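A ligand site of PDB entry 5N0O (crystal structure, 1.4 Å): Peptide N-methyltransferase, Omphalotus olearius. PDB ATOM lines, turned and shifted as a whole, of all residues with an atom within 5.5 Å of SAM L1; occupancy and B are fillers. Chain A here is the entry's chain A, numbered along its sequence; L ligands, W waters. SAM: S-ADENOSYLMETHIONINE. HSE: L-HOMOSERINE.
The backbone NH (N) of Tyr 210 lies within hydrogen-bond range of the backbone carbonyl oxygen (O) of Thr 244, 2.9 Å away.
The side-chain hydroxyl of Ser 243 sits at hydrogen-bond distance from the backbone NH of Gly 240.
OG of Ser 128 is in hydrogen-bond range of N of Glu 130, 3.1 Å away.
The backbone carbonyl oxygen of Tyr 97 is in hydrogen-bond range of a nitrogen (N) of SAM L1.
The backbone NH (N) of Ala 212 lies within hydrogen-bond range of a nitrogen (N1) of SAM L1.
O of Ala 212 is in hydrogen-bond range of N6 of SAM L1, at 3.1 Å.
A nitrogen (N) of HSE L2 sits at hydrogen-bond distance from the side-chain amide oxygen of Gln 171, 2.9 Å away.
The backbone NH of Ala 129 sits at hydrogen-bond distance from an oxygen (O) of SAM L1 (2.9 Å).
The side-chain hydroxyl of Thr 244 is in hydrogen-bond range of an oxygen (O2') of SAM L1 (2.8 Å).
O2' of SAM L1 lies within hydrogen-bond range of N of Gln 171, 3.0 Å away.
A nitrogen (N) of SAM L1 lies within hydrogen-bond range of the backbone carbonyl oxygen of Val 102 (2.8 Å).
The backbone carbonyl oxygen (O) of Ser 243 sits at hydrogen-bond distance from an oxygen (O2') of SAM L1 (3.2 Å).
O of His 99 sits at hydrogen-bond distance from N of SAM L1 (3.0 Å).
OXT of SAM L1 is in hydrogen-bond range of N of His 99.
O of Gly 241 is in hydrogen-bond range of O3' of SAM L1 (3.3 Å).
A sulfur (SD) of SAM L1 lies close to the backbone carbonyl oxygen (O) of Phe 103 (3.3 Å).
The backbone carbonyl oxygen (O) of Val 242 sits close to a nitrogen (N3) of SAM L1.
Ile 18 touches SAM L1 (CG2 to N6, 3.6 Å).
Gly 98 touches SAM L1.
Val 104 touches SAM L1.
CA of Ser 128 touches OXT of SAM L1, 3.4 Å away.
CA of Phe 170 touches O2' of SAM L1, 3.3 Å away.
Tyr 210 touches SAM L1 (O to C2, 3.6 Å).
CA of Ile 211 touches N1 of SAM L1, at 3.5 Å.
Hydrophobic or aromatic side chains within 4 Å of SAM L1: Ile 18, Tyr 97, His 99, Val 102, Phe 103, Val 104, Ala 129, Phe 170, Tyr 210, Ala 212 and Val 242.
18 residues have an atom within 4 Å of SAM L1: Ile 18, Tyr 97, Gly 98, His 99, Val 102, Phe 103, Val 104, Ser 128, Ala 129, Phe 170, Gln 171, Tyr 210, Ile 211, Ala 212, Gly 241, Val 242, Ser 243 and Thr 244.
Along chain A the residues within 4 Å of SAM L1 span positions 18 to 244.
The nearest printed residue that does not touch SAM L1 is Val 127 (4.5 Å).
Water W2 bridges the backbone carbonyl oxygen of Tyr 97 (2.7 Å) and a nitrogen (N) of SAM L1 (2.9 Å).
Water W3 lies within hydrogen-bond range of the backbone carbonyl oxygen of Ser 243, the backbone carbonyl oxygen of Gly 240, an oxygen (O3') of SAM L1 and the backbone NH of Val 172.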
ATOM      1  N   ILE A  18      14.692   0.463 -11.191  1.00  0.00           N
ATOM      2  CA  ILE A  18      13.887   0.098 -12.375  1.00  0.00           C
ATOM      3  C   ILE A  18      14.759  -0.183 -13.607  1.00  0.00           C
ATOM      4  O   ILE A  18      14.596  -1.217 -14.276  1.00  0.00           O
ATOM      5  CB  ILE A  18      12.799   1.186 -12.654  1.00  0.00           C
ATOM      6  CG1 ILE A  18      11.832   1.330 -11.462  1.00  0.00           C
ATOM      7  CG2 ILE A  18      12.048   0.880 -13.939  1.00  0.00           C
ATOM      8  CD1 ILE A  18      10.996   0.103 -11.152  1.00  0.00           C
ATOM      9  N   ILE A  43      12.571  -8.381 -13.253  1.00  0.00           N
ATOM     10  CA  ILE A  43      11.907  -8.602 -14.544  1.00  0.00           C
ATOM     11  C   ILE A  43      12.755  -8.167 -15.750  1.00  0.00           C
ATOM     12  O   ILE A  43      12.197  -7.948 -16.830  1.00  0.00           O
ATOM     13  CB  ILE A  43      10.473  -7.981 -14.520  1.00  0.00           C
ATOM     14  CG1 ILE A  43      10.527  -6.490 -14.151  1.00  0.00           C
ATOM     15  CG2 ILE A  43       9.600  -8.722 -13.522  1.00  0.00           C
ATOM     16  CD1 ILE A  43       9.215  -5.755 -14.380  1.00  0.00           C
ATOM     17  N   TYR A  97      12.622  -5.874  -7.594  1.00  0.00           N
ATOM     18  CA  TYR A  97      12.893  -4.741  -8.478  1.00  0.00           C
ATOM     19  C   TYR A  97      12.242  -3.442  -7.954  1.00  0.00           C
ATOM     20  O   TYR A  97      11.208  -3.461  -7.258  1.00  0.00           O
ATOM     21  CB  TYR A  97      12.517  -5.035  -9.938  1.00  0.00           C
ATOM     22  CG  TYR A  97      11.051  -4.952 -10.288  1.00  0.00           C
ATOM     23  CD1 TYR A  97      10.193  -6.042 -10.187  1.00  0.00           C
ATOM     24  CD2 TYR A  97      10.524  -3.746 -10.771  1.00  0.00           C
ATOM     25  CE1 TYR A  97       8.841  -5.936 -10.532  1.00  0.00           C
ATOM     26  CE2 TYR A  97       9.194  -3.631 -11.109  1.00  0.00           C
ATOM     27  CZ  TYR A  97       8.358  -4.712 -10.991  1.00  0.00           C
ATOM     28  OH  TYR A  97       7.026  -4.578 -11.360  1.00  0.00           O
ATOM     29  N   GLY A  98      12.868  -2.302  -8.273  1.00  0.00           N
ATOM     30  CA  GLY A  98      12.384  -0.998  -7.800  1.00  0.00           C
ATOM     31  C   GLY A  98      12.766  -0.755  -6.347  1.00  0.00           C
ATOM     32  O   GLY A  98      13.899  -1.043  -5.934  1.00  0.00           O
ATOM     33  N   HIS A  99      11.813  -0.212  -5.576  1.00  0.00           N
ATOM     34  CA  HIS A  99      11.871  -0.126  -4.105  1.00  0.00           C
ATOM     35  C   HIS A  99      11.116  -1.365  -3.603  1.00  0.00           C
ATOM     36  O   HIS A  99       9.972  -1.610  -4.019  1.00  0.00           O
ATOM     37  CB  HIS A  99      11.172   1.170  -3.657  1.00  0.00           C
ATOM     38  CG  HIS A  99      11.166   1.452  -2.171  1.00  0.00           C
ATOM     39  ND1 HIS A  99      10.730   0.557  -1.214  1.00  0.00           N
ATOM     40  CD2 HIS A  99      11.438   2.599  -1.502  1.00  0.00           C
ATOM     41  CE1 HIS A  99      10.775   1.126  -0.016  1.00  0.00           C
ATOM     42  NE2 HIS A  99      11.186   2.373  -0.167  1.00  0.00           N
ATOM     43  N   PRO A 100      11.739  -2.165  -2.714  1.00  0.00           N
ATOM     44  CA  PRO A 100      11.139  -3.453  -2.337  1.00  0.00           C
ATOM     45  C   PRO A 100       9.878  -3.403  -1.458  1.00  0.00           C
ATOM     46  O   PRO A 100       9.300  -4.471  -1.209  1.00  0.00           O
ATOM     47  CB  PRO A 100      12.287  -4.140  -1.607  1.00  0.00           C
ATOM     48  CG  PRO A 100      13.031  -3.006  -0.951  1.00  0.00           C
ATOM     49  CD  PRO A 100      12.992  -1.913  -1.968  1.00  0.00           C
ATOM     50  N   VAL A 102       7.375  -0.758  -2.090  1.00  0.00           N
ATOM     51  CA  VAL A 102       6.442   0.106  -2.816  1.00  0.00           C
ATOM     52  C   VAL A 102       5.613  -0.783  -3.770  1.00  0.00           C
ATOM     53  O   VAL A 102       6.130  -1.294  -4.765  1.00  0.00           O
ATOM     54  CB  VAL A 102       7.224   1.235  -3.546  1.00  0.00           C
ATOM     55  CG1 VAL A 102       6.362   1.983  -4.545  1.00  0.00           C
ATOM     56  CG2 VAL A 102       7.804   2.216  -2.529  1.00  0.00           C
ATOM     57  N   PHE A 103       4.333  -0.955  -3.459  1.00  0.00           N
ATOM     58  CA  PHE A 103       3.437  -1.882  -4.172  1.00  0.00           C
ATOM     59  C   PHE A 103       4.008  -3.312  -4.224  1.00  0.00           C
ATOM     60  O   PHE A 103       4.013  -3.963  -5.281  1.00  0.00           O
ATOM     61  CB  PHE A 103       3.034  -1.314  -5.555  1.00  0.00           C
ATOM     62  CG  PHE A 103       2.261  -0.021  -5.491  1.00  0.00           C
ATOM     63  CD1 PHE A 103       2.904   1.189  -5.252  1.00  0.00           C
ATOM     64  CD2 PHE A 103       0.873   0.001  -5.654  1.00  0.00           C
ATOM     65  CE1 PHE A 103       2.197   2.379  -5.168  1.00  0.00           C
ATOM     66  CE2 PHE A 103       0.176   1.190  -5.561  1.00  0.00           C
ATOM     67  CZ  PHE A 103       0.828   2.380  -5.323  1.00  0.00           C
ATOM     68  N   VAL A 104       4.502  -3.793  -3.079  1.00  0.00           N
ATOM     69  CA  VAL A 104       5.022  -5.172  -2.906  1.00  0.00           C
ATOM     70  C   VAL A 104       4.487  -5.772  -1.593  1.00  0.00           C
ATOM     71  O   VAL A 104       4.842  -5.324  -0.514  1.00  0.00           O
ATOM     72  CB  VAL A 104       6.577  -5.214  -2.872  1.00  0.00           C
ATOM     73  CG1 VAL A 104       7.089  -6.636  -2.736  1.00  0.00           C
ATOM     74  CG2 VAL A 104       7.186  -4.563  -4.105  1.00  0.00           C
ATOM     75  N   VAL A 127      15.037   2.796  -5.585  1.00  0.00           N
ATOM     76  CA  VAL A 127      14.444   3.709  -6.555  1.00  0.00           C
ATOM     77  C   VAL A 127      13.170   3.097  -7.154  1.00  0.00           C
ATOM     78  O   VAL A 127      13.239   2.057  -7.829  1.00  0.00           O
ATOM     79  CB  VAL A 127      15.468   4.069  -7.666  1.00  0.00           C
ATOM     80  CG1 VAL A 127      14.826   4.926  -8.759  1.00  0.00           C
ATOM     81  CG2 VAL A 127      16.705   4.763  -7.079  1.00  0.00           C
ATOM     82  N   SER A 128      12.023   3.715  -6.911  1.00  0.00           N
ATOM     83  CA  SER A 128      10.730   3.185  -7.381  1.00  0.00           C
ATOM     84  C   SER A 128      10.340   3.680  -8.781  1.00  0.00           C
ATOM     85  O   SER A 128      10.937   4.625  -9.327  1.00  0.00           O
ATOM     86  CB  SER A 128       9.606   3.584  -6.420  1.00  0.00           C
ATOM     87  OG  SER A 128       9.223   4.942  -6.617  1.00  0.00           O
ATOM     88  N   ALA A 129       9.276   3.098  -9.336  1.00  0.00           N
ATOM     89  CA  ALA A 129       8.721   3.605 -10.596  1.00  0.00           C
ATOM     90  C   ALA A 129       8.189   5.047 -10.469  1.00  0.00           C
ATOM     91  O   ALA A 129       8.206   5.787 -11.458  1.00  0.00           O
ATOM     92  CB  ALA A 129       7.632   2.665 -11.124  1.00  0.00           C
ATOM     93  N   GLU A 130       7.714   5.439  -9.280  1.00  0.00           N
ATOM     94  CA  GLU A 130       7.302   6.831  -9.042  1.00  0.00           C
ATOM     95  C   GLU A 130       8.514   7.784  -9.044  1.00  0.00           C
ATOM     96  O   GLU A 130       8.435   8.894  -9.603  1.00  0.00           O
ATOM     97  CB  GLU A 130       6.465   6.973  -7.764  1.00  0.00           C
ATOM     98  CG  GLU A 130       5.947   8.407  -7.597  1.00  0.00           C
ATOM     99  CD  GLU A 130       4.878   8.579  -6.526  1.00  0.00           C
ATOM    100  OE1 GLU A 130       5.236   8.793  -5.351  1.00  0.00           O
ATOM    101  OE2 GLU A 130       3.675   8.543  -6.889  1.00  0.00           O
ATOM    102  N   LEU A 169      -1.351   6.715 -10.654  1.00  0.00           N
ATOM    103  CA  LEU A 169      -2.059   5.417 -10.506  1.00  0.00           C
ATOM    104  C   LEU A 169      -1.180   4.248 -10.965  1.00  0.00           C
ATOM    105  O   LEU A 169      -0.780   4.193 -12.147  1.00  0.00           O
ATOM    106  CB  LEU A 169      -3.398   5.399 -11.288  1.00  0.00           C
ATOM    107  CG  LEU A 169      -4.446   6.463 -10.915  1.00  0.00           C
ATOM    108  CD1 LEU A 169      -5.658   6.336 -11.835  1.00  0.00           C
ATOM    109  CD2 LEU A 169      -4.880   6.348  -9.465  1.00  0.00           C
ATOM    110  N   PHE A 170      -0.842   3.349 -10.036  1.00  0.00           N
ATOM    111  CA  PHE A 170      -0.100   2.102 -10.312  1.00  0.00           C
ATOM    112  C   PHE A 170      -1.085   0.975 -10.688  1.00  0.00           C
ATOM    113  O   PHE A 170      -2.259   0.995 -10.280  1.00  0.00           O
ATOM    114  CB  PHE A 170       0.686   1.618  -9.079  1.00  0.00           C
ATOM    115  CG  PHE A 170       2.009   2.312  -8.815  1.00  0.00           C
ATOM    116  CD1 PHE A 170       2.091   3.660  -8.459  1.00  0.00           C
ATOM    117  CD2 PHE A 170       3.193   1.568  -8.822  1.00  0.00           C
ATOM    118  CE1 PHE A 170       3.328   4.251  -8.168  1.00  0.00           C
ATOM    119  CE2 PHE A 170       4.430   2.149  -8.529  1.00  0.00           C
ATOM    120  CZ  PHE A 170       4.487   3.496  -8.212  1.00  0.00           C
ATOM    121  N   GLN A 171      -0.595  -0.036 -11.404  1.00  0.00           N
ATOM    122  CA  GLN A 171      -1.383  -1.268 -11.664  1.00  0.00           C
ATOM    123  C   GLN A 171      -2.676  -1.020 -12.479  1.00  0.00           C
ATOM    124  O   GLN A 171      -3.680  -1.724 -12.316  1.00  0.00           O
ATOM    125  CB  GLN A 171      -1.573  -2.093 -10.357  1.00  0.00           C
ATOM    126  CG  GLN A 171      -0.207  -2.493  -9.772  1.00  0.00           C
ATOM    127  CD  GLN A 171      -0.206  -3.484  -8.627  1.00  0.00           C
ATOM    128  OE1 GLN A 171       0.867  -3.981  -8.254  1.00  0.00           O
ATOM    129  NE2 GLN A 171      -1.369  -3.787  -8.079  1.00  0.00           N
ATOM    130  N   VAL A 172      -2.594  -0.059 -13.400  1.00  0.00           N
ATOM    131  CA  VAL A 172      -3.686   0.236 -14.352  1.00  0.00           C
ATOM    132  C   VAL A 172      -3.867  -0.884 -15.397  1.00  0.00           C
ATOM    133  O   VAL A 172      -4.914  -0.934 -16.069  1.00  0.00           O
ATOM    134  CB  VAL A 172      -3.498   1.609 -15.050  1.00  0.00           C
ATOM    135  CG1 VAL A 172      -3.592   2.755 -14.046  1.00  0.00           C
ATOM    136  CG2 VAL A 172      -2.183   1.694 -15.814  1.00  0.00           C
ATOM    137  N   TYR A 210       2.779   6.175 -18.896  1.00  0.00           N
ATOM    138  CA  TYR A 210       4.202   6.176 -18.536  1.00  0.00           C
ATOM    139  C   TYR A 210       4.769   4.753 -18.356  1.00  0.00           C
ATOM    140  O   TYR A 210       4.246   3.975 -17.538  1.00  0.00           O
ATOM    141  CB  TYR A 210       4.447   6.988 -17.247  1.00  0.00           C
ATOM    142  CG  TYR A 210       5.897   6.983 -16.809  1.00  0.00           C
ATOM    143  CD1 TYR A 210       6.880   7.550 -17.616  1.00  0.00           C
ATOM    144  CD2 TYR A 210       6.295   6.371 -15.624  1.00  0.00           C
ATOM    145  CE1 TYR A 210       8.222   7.528 -17.236  1.00  0.00           C
ATOM    146  CE2 TYR A 210       7.636   6.338 -15.243  1.00  0.00           C
ATOM    147  CZ  TYR A 210       8.599   6.907 -16.048  1.00  0.00           C
ATOM    148  OH  TYR A 210       9.914   6.888 -15.644  1.00  0.00           O
ATOM    149  N   ILE A 211       5.834   4.455 -19.106  1.00  0.00           N
ATOM    150  CA  ILE A 211       6.663   3.238 -18.899  1.00  0.00           C
ATOM    151  C   ILE A 211       8.123   3.675 -18.855  1.00  0.00           C
ATOM    152  O   ILE A 211       8.688   4.094 -19.876  1.00  0.00           O
ATOM    153  CB  ILE A 211       6.461   2.147 -19.973  1.00  0.00           C
ATOM    154  CG1 ILE A 211       4.977   1.799 -20.192  1.00  0.00           C
ATOM    155  CG2 ILE A 211       7.246   0.877 -19.576  1.00  0.00           C
ATOM    156  CD1 ILE A 211       4.697   0.877 -21.359  1.00  0.00           C
ATOM    157  N   ALA A 212       8.743   3.601 -17.671  1.00  0.00           N
ATOM    158  CA  ALA A 212      10.185   3.877 -17.503  1.00  0.00           C
ATOM    159  C   ALA A 212      10.988   2.869 -18.306  1.00  0.00           C
ATOM    160  O   ALA A 212      10.639   1.691 -18.379  1.00  0.00           O
ATOM    161  CB  ALA A 212      10.602   3.777 -16.042  1.00  0.00           C
ATOM    162  N   ALA A 213      12.066   3.353 -18.927  1.00  0.00           N
ATOM    163  CA  ALA A 213      12.967   2.454 -19.648  1.00  0.00           C
ATOM    164  C   ALA A 213      13.620   1.425 -18.697  1.00  0.00           C
ATOM    165  O   ALA A 213      14.070   1.777 -17.612  1.00  0.00           O
ATOM    166  CB  ALA A 213      14.048   3.252 -20.371  1.00  0.00           C
ATOM    167  N   MET A 214      13.648   0.165 -19.131  1.00  0.00           N
ATOM    168  CA  MET A 214      14.310  -0.878 -18.362  1.00  0.00           C
ATOM    169  C   MET A 214      15.749  -1.015 -18.761  1.00  0.00           C
ATOM    170  O   MET A 214      16.605  -1.211 -17.909  1.00  0.00           O
ATOM    171  CB  MET A 214      13.590  -2.192 -18.584  1.00  0.00           C
ATOM    172  CG  MET A 214      13.992  -3.217 -17.534  1.00  0.00           C
ATOM    173  SD  MET A 214      12.966  -4.859 -17.841  1.00  0.00           S
ATOM    174  CE  MET A 214      11.292  -4.054 -17.196  1.00  0.00           C
ATOM    175  N   GLY A 240      -0.181  -2.233 -20.184  1.00  0.00           N
ATOM    176  CA  GLY A 240       0.246  -3.553 -19.702  1.00  0.00           C
ATOM    177  C   GLY A 240       0.716  -3.588 -18.261  1.00  0.00           C
ATOM    178  O   GLY A 240       0.418  -2.695 -17.468  1.00  0.00           O
ATOM    179  N   GLY A 241       1.482  -4.620 -17.928  1.00  0.00           N
ATOM    180  CA  GLY A 241       1.906  -4.889 -16.557  1.00  0.00           C
ATOM    181  C   GLY A 241       2.942  -3.959 -15.952  1.00  0.00           C
ATOM    182  O   GLY A 241       3.138  -3.972 -14.723  1.00  0.00           O
ATOM    183  N   VAL A 242       3.644  -3.185 -16.791  1.00  0.00           N
ATOM    184  CA  VAL A 242       4.621  -2.190 -16.304  1.00  0.00           C
ATOM    185  C   VAL A 242       4.174  -0.734 -16.601  1.00  0.00           C
ATOM    186  O   VAL A 242       5.006   0.182 -16.637  1.00  0.00           O
ATOM    187  CB  VAL A 242       6.067  -2.476 -16.806  1.00  0.00           C
ATOM    188  CG1 VAL A 242       6.590  -3.748 -16.136  1.00  0.00           C
ATOM    189  CG2 VAL A 242       6.143  -2.593 -18.320  1.00  0.00           C
ATOM    190  N   SER A 243       2.872  -0.542 -16.826  1.00  0.00           N
ATOM    191  CA  SER A 243       2.284   0.782 -17.119  1.00  0.00           C
ATOM    192  C   SER A 243       1.793   1.502 -15.858  1.00  0.00           C
ATOM    193  O   SER A 243       1.134   0.887 -15.005  1.00  0.00           O
ATOM    194  CB  SER A 243       1.088   0.632 -18.070  1.00  0.00           C
ATOM    195  OG  SER A 243       1.473   0.158 -19.364  1.00  0.00           O
ATOM    196  N   THR A 244       2.103   2.794 -15.768  1.00  0.00           N
ATOM    197  CA  THR A 244       1.611   3.671 -14.700  1.00  0.00           C
ATOM    198  C   THR A 244       0.953   4.891 -15.381  1.00  0.00           C
ATOM    199  O   THR A 244       1.388   5.304 -16.467  1.00  0.00           O
ATOM    200  CB  THR A 244       2.785   4.082 -13.774  1.00  0.00           C
ATOM    201  OG1 THR A 244       3.275   2.903 -13.097  1.00  0.00           O
ATOM    202  CG2 THR A 244       2.405   5.111 -12.719  1.00  0.00           C
HETATM  203  N   SAM L   1       8.270  -2.185  -6.417  1.00  0.00           N
HETATM  204  CA  SAM L   1       7.940  -1.585  -7.710  1.00  0.00           C
HETATM  205  C   SAM L   1       8.415  -0.129  -7.700  1.00  0.00           C
HETATM  206  O   SAM L   1       7.966   0.671  -8.569  1.00  0.00           O
HETATM  207  OXT SAM L   1       9.236   0.232  -6.820  1.00  0.00           O
HETATM  208  CB  SAM L   1       6.435  -1.732  -8.080  1.00  0.00           C
HETATM  209  CG  SAM L   1       5.817  -3.180  -8.114  1.00  0.00           C
HETATM  210  SD  SAM L   1       4.143  -3.407  -8.500  1.00  0.00           S
HETATM  211  CE  SAM L   1       3.913  -5.042  -8.264  1.00  0.00           C
HETATM  212  C5' SAM L   1       3.948  -3.228 -10.195  1.00  0.00           C
HETATM  213  C4' SAM L   1       3.536  -1.846 -10.763  1.00  0.00           C
HETATM  214  O4' SAM L   1       4.671  -0.968 -10.772  1.00  0.00           O
HETATM  215  C3' SAM L   1       3.047  -1.789 -12.214  1.00  0.00           C
HETATM  216  O3' SAM L   1       1.666  -2.172 -12.391  1.00  0.00           O
HETATM  217  C2' SAM L   1       3.300  -0.326 -12.572  1.00  0.00           C
HETATM  218  O2' SAM L   1       2.272   0.536 -12.056  1.00  0.00           O
HETATM  219  C1' SAM L   1       4.605  -0.028 -11.835  1.00  0.00           C
HETATM  220  N9  SAM L   1       5.794  -0.233 -12.706  1.00  0.00           N
HETATM  221  C8  SAM L   1       6.651  -1.297 -12.715  1.00  0.00           C
HETATM  222  N7  SAM L   1       7.628  -1.141 -13.655  1.00  0.00           N
HETATM  223  C5  SAM L   1       7.379   0.057 -14.261  1.00  0.00           C
HETATM  224  C6  SAM L   1       8.002   0.818 -15.352  1.00  0.00           C
HETATM  225  N6  SAM L   1       9.097   0.365 -15.994  1.00  0.00           N
HETATM  226  N1  SAM L   1       7.444   2.019 -15.660  1.00  0.00           N
HETATM  227  C2  SAM L   1       6.337   2.482 -15.038  1.00  0.00           C
HETATM  228  N3  SAM L   1       5.711   1.833 -14.054  1.00  0.00           N
HETATM  229  C4  SAM L   1       6.192   0.636 -13.627  1.00  0.00           C
HETATM  230  N   HSE L   2       1.314  -6.837  -8.278  1.00  0.00           N
HETATM  231  CA  HSE L   2       1.254  -7.883  -9.281  1.00  0.00           C
HETATM  232  C   HSE L   2       2.557  -8.655  -9.290  1.00  0.00           C
HETATM  233  C3  HSE L   2       0.819  -7.352 -10.658  1.00  0.00           C
HETATM  234  O   HSE L   2       3.305  -8.629 -10.296  1.00  0.00           O
HETATM  235  OXT HSE L   2       2.831  -9.321  -8.268  1.00  0.00           O
HETATM  236  C4  HSE L   2       1.485  -6.053 -11.094  1.00  0.00           C
HETATM  237  O3  HSE L   2       1.044  -5.688 -12.409  1.00  0.00           O
HETATM  238  O   HOH W   1      10.027  -2.242 -14.647  1.00  0.00           O
HETATM  239  O   HOH W   2       8.907  -4.914  -6.995  1.00  0.00           O
HETATM  240  O   HOH W   3       0.096  -1.661 -14.796  1.00  0.00           O
